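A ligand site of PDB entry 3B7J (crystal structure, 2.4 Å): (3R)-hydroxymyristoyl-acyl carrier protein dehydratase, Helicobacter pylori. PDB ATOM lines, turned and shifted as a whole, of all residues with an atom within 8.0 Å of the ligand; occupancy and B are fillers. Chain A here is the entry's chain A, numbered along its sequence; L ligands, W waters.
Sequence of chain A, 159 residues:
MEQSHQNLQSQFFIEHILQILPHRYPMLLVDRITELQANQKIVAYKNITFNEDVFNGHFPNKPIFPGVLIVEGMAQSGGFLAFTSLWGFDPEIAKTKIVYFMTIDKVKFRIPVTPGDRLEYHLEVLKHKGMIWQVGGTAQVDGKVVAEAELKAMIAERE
A nitrogen (N2) of the ligand lies close to the side-chain amide nitrogen of Gln 40 (2.7 Å). OE2 of Glu 124 lies within salt-bridge range of N1 of the ligand, at 2.9 Å.
O of Gln 40 is in hydrogen-bond range of N of Val 125, at 2.8 Å. The backbone NH (N) of Glu 124 is in hydrogen-bond range of the backbone carbonyl oxygen (O) of Gly 136, at 2.8 Å.
Residues that only touch the ligand: Val 125 (3.4 Å). Three residues have an atom within 4 Å of the ligand: Gln 40, Glu 124 and Val 125. The nearest printed residue that does not touch the ligand is Lys 41 (4.04 Å).
Water W1 lies within hydrogen-bond range of the side-chain amide nitrogen (NE2) of Gln 40 (2.7 Å) and a nitrogen (N1) of the ligand (3.0 Å).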
ATOM      1  N   GLN A  37     -13.251   0.308   3.000  1.00  0.00           N
ATOM      2  CA  GLN A  37     -13.530   0.139   4.417  1.00  0.00           C
ATOM      3  C   GLN A  37     -12.699   1.189   5.154  1.00  0.00           C
ATOM      4  O   GLN A  37     -11.466   1.108   5.209  1.00  0.00           O
ATOM      5  CB  GLN A  37     -13.118  -1.265   4.887  1.00  0.00           C
ATOM      6  CG  GLN A  37     -13.717  -1.645   6.237  1.00  0.00           C
ATOM      7  CD  GLN A  37     -15.251  -1.803   6.172  1.00  0.00           C
ATOM      8  OE1 GLN A  37     -15.955  -1.651   7.184  1.00  0.00           O
ATOM      9  NE2 GLN A  37     -15.765  -2.119   4.972  1.00  0.00           N
ATOM     10  N   ALA A  38     -13.378   2.190   5.710  1.00  0.00           N
ATOM     11  CA  ALA A  38     -12.722   3.277   6.429  1.00  0.00           C
ATOM     12  C   ALA A  38     -11.617   2.799   7.376  1.00  0.00           C
ATOM     13  O   ALA A  38     -11.807   1.843   8.129  1.00  0.00           O
ATOM     14  CB  ALA A  38     -13.752   4.078   7.204  1.00  0.00           C
ATOM     15  N   ASN A  39     -10.470   3.464   7.324  1.00  0.00           N
ATOM     16  CA  ASN A  39      -9.318   3.160   8.175  1.00  0.00           C
ATOM     17  C   ASN A  39      -8.719   1.767   7.986  1.00  0.00           C
ATOM     18  O   ASN A  39      -7.740   1.422   8.644  1.00  0.00           O
ATOM     19  CB  ASN A  39      -9.681   3.313   9.649  1.00  0.00           C
ATOM     20  CG  ASN A  39     -10.285   4.651   9.963  1.00  0.00           C
ATOM     21  OD1 ASN A  39     -11.299   4.738  10.649  1.00  0.00           O
ATOM     22  ND2 ASN A  39      -9.671   5.714   9.466  1.00  0.00           N
ATOM     23  N   GLN A  40      -9.262   0.979   7.077  1.00  0.00           N
ATOM     24  CA  GLN A  40      -8.755  -0.375   6.896  1.00  0.00           C
ATOM     25  C   GLN A  40      -8.243  -0.661   5.500  1.00  0.00           C
ATOM     26  O   GLN A  40      -7.091  -1.045   5.333  1.00  0.00           O
ATOM     27  CB  GLN A  40      -9.791  -1.441   7.279  1.00  0.00           C
ATOM     28  CG  GLN A  40      -9.915  -1.656   8.784  1.00  0.00           C
ATOM     29  CD  GLN A  40     -10.746  -2.866   9.122  1.00  0.00           C
ATOM     30  OE1 GLN A  40     -11.849  -2.748   9.650  1.00  0.00           O
ATOM     31  NE2 GLN A  40     -10.231  -4.052   8.808  1.00  0.00           N
ATOM     32  N   LYS A  41      -9.076  -0.476   4.481  1.00  0.00           N
ATOM     33  CA  LYS A  41      -8.623  -0.749   3.142  1.00  0.00           C
ATOM     34  C   LYS A  41      -9.483  -0.230   2.010  1.00  0.00           C
ATOM     35  O   LYS A  41     -10.587   0.302   2.193  1.00  0.00           O
ATOM     36  CB  LYS A  41      -8.477  -2.250   2.943  1.00  0.00           C
ATOM     37  CG  LYS A  41      -9.779  -2.991   2.868  1.00  0.00           C
ATOM     38  CD  LYS A  41      -9.555  -4.349   2.231  1.00  0.00           C
ATOM     39  CE  LYS A  41     -10.831  -5.169   2.170  1.00  0.00           C
ATOM     40  NZ  LYS A  41     -10.531  -6.466   1.476  1.00  0.00           N
ATOM     41  N   ILE A  42      -8.926  -0.405   0.811  1.00  0.00           N
ATOM     42  CA  ILE A  42      -9.579  -0.007  -0.411  1.00  0.00           C
ATOM     43  C   ILE A  42      -9.103  -0.916  -1.542  1.00  0.00           C
ATOM     44  O   ILE A  42      -7.948  -1.357  -1.572  1.00  0.00           O
ATOM     45  CB  ILE A  42      -9.251   1.457  -0.756  1.00  0.00           C
ATOM     46  CG1 ILE A  42      -9.980   1.855  -2.042  1.00  0.00           C
ATOM     47  CG2 ILE A  42      -7.758   1.647  -0.896  1.00  0.00           C
ATOM     48  CD1 ILE A  42      -9.936   3.331  -2.334  1.00  0.00           C
ATOM     49  N   LEU A 123      -4.945  -1.750  -1.470  1.00  0.00           N
ATOM     50  CA  LEU A 123      -4.218  -1.056  -0.417  1.00  0.00           C
ATOM     51  C   LEU A 123      -4.832  -1.315   0.955  1.00  0.00           C
ATOM     52  O   LEU A 123      -6.044  -1.450   1.087  1.00  0.00           O
ATOM     53  CB  LEU A 123      -4.212   0.467  -0.674  1.00  0.00           C
ATOM     54  CG  LEU A 123      -3.241   1.010  -1.737  1.00  0.00           C
ATOM     55  CD1 LEU A 123      -1.815   0.712  -1.311  1.00  0.00           C
ATOM     56  CD2 LEU A 123      -3.523   0.372  -3.094  1.00  0.00           C
ATOM     57  N   GLU A 124      -3.975  -1.390   1.954  1.00  0.00           N
ATOM     58  CA  GLU A 124      -4.429  -1.614   3.312  1.00  0.00           C
ATOM     59  C   GLU A 124      -3.678  -0.651   4.256  1.00  0.00           C
ATOM     60  O   GLU A 124      -2.522  -0.319   4.021  1.00  0.00           O
ATOM     61  CB  GLU A 124      -4.249  -3.084   3.680  1.00  0.00           C
ATOM     62  CG  GLU A 124      -5.052  -3.978   2.710  1.00  0.00           C
ATOM     63  CD  GLU A 124      -5.334  -5.375   3.213  1.00  0.00           C
ATOM     64  OE1 GLU A 124      -4.401  -6.213   3.247  1.00  0.00           O
ATOM     65  OE2 GLU A 124      -6.511  -5.638   3.572  1.00  0.00           O
ATOM     66  N   VAL A 125      -4.377  -0.192   5.284  1.00  0.00           N
ATOM     67  CA  VAL A 125      -3.819   0.748   6.247  1.00  0.00           C
ATOM     68  C   VAL A 125      -2.913   0.074   7.276  1.00  0.00           C
ATOM     69  O   VAL A 125      -3.354  -0.753   8.082  1.00  0.00           O
ATOM     70  CB  VAL A 125      -4.941   1.503   6.983  1.00  0.00           C
ATOM     71  CG1 VAL A 125      -4.349   2.484   7.987  1.00  0.00           C
ATOM     72  CG2 VAL A 125      -5.831   2.213   5.962  1.00  0.00           C
ATOM     73  N   LEU A 126      -1.633   0.422   7.233  1.00  0.00           N
ATOM     74  CA  LEU A 126      -0.666  -0.145   8.149  1.00  0.00           C
ATOM     75  C   LEU A 126      -0.570   0.688   9.424  1.00  0.00           C
ATOM     76  O   LEU A 126      -0.351   0.142  10.512  1.00  0.00           O
ATOM     77  CB  LEU A 126       0.696  -0.228   7.459  1.00  0.00           C
ATOM     78  CG  LEU A 126       0.716  -1.131   6.205  1.00  0.00           C
ATOM     79  CD1 LEU A 126       2.042  -0.975   5.479  1.00  0.00           C
ATOM     80  CD2 LEU A 126       0.504  -2.582   6.617  1.00  0.00           C
ATOM     81  N   LYS A 127      -0.759   1.992   9.284  1.00  0.00           N
ATOM     82  CA  LYS A 127      -0.698   2.901  10.421  1.00  0.00           C
ATOM     83  C   LYS A 127      -1.243   4.294  10.057  1.00  0.00           C
ATOM     84  O   LYS A 127      -0.972   4.820   8.991  1.00  0.00           O
ATOM     85  CB  LYS A 127       0.746   2.992  10.909  1.00  0.00           C
ATOM     86  CG  LYS A 127       0.972   3.873  12.124  1.00  0.00           C
ATOM     87  CD  LYS A 127       2.296   3.505  12.809  1.00  0.00           C
ATOM     88  CE  LYS A 127       2.698   4.539  13.834  1.00  0.00           C
ATOM     89  NZ  LYS A 127       2.980   5.826  13.141  1.00  0.00           N
ATOM     90  N   GLN A 134       0.158   5.446   6.513  1.00  0.00           N
ATOM     91  CA  GLN A 134       1.072   4.463   5.950  1.00  0.00           C
ATOM     92  C   GLN A 134       0.228   3.336   5.398  1.00  0.00           C
ATOM     93  O   GLN A 134      -0.492   2.669   6.146  1.00  0.00           O
ATOM     94  CB  GLN A 134       2.019   3.925   7.023  1.00  0.00           C
ATOM     95  CG  GLN A 134       3.095   4.904   7.410  1.00  0.00           C
ATOM     96  CD  GLN A 134       3.790   4.541   8.709  1.00  0.00           C
ATOM     97  OE1 GLN A 134       4.321   3.438   8.857  1.00  0.00           O
ATOM     98  NE2 GLN A 134       3.787   5.473   9.670  1.00  0.00           N
ATOM     99  N   GLY A 136       0.032  -0.073   2.511  1.00  0.00           N
ATOM    100  CA  GLY A 136       0.833  -1.045   1.810  1.00  0.00           C
ATOM    101  C   GLY A 136      -0.113  -1.964   1.092  1.00  0.00           C
ATOM    102  O   GLY A 136      -1.268  -2.112   1.501  1.00  0.00           O
HETATM  103  C1  LIG L   1      -5.696  -4.707   7.006  1.00  0.00           C
HETATM  104  C2  LIG L   1      -4.856  -3.873   7.741  1.00  0.00           C
HETATM  105  C3  LIG L   1      -3.485  -4.116   7.781  1.00  0.00           C
HETATM  106  C4  LIG L   1      -2.963  -5.195   7.081  1.00  0.00           C
HETATM  107  C5  LIG L   1      -3.802  -6.023   6.338  1.00  0.00           C
HETATM  108  C6  LIG L   1      -5.165  -5.777   6.302  1.00  0.00           C
HETATM  109  C7  LIG L   1      -7.072  -4.507   7.035  1.00  0.00           C
HETATM  110  N1  LIG L   1      -7.811  -4.835   5.981  1.00  0.00           N
HETATM  111  N2  LIG L   1      -7.643  -4.014   8.136  1.00  0.00           N
HETATM  112  O   HOH W   1     -10.831  -4.513   6.229  1.00  0.00           O
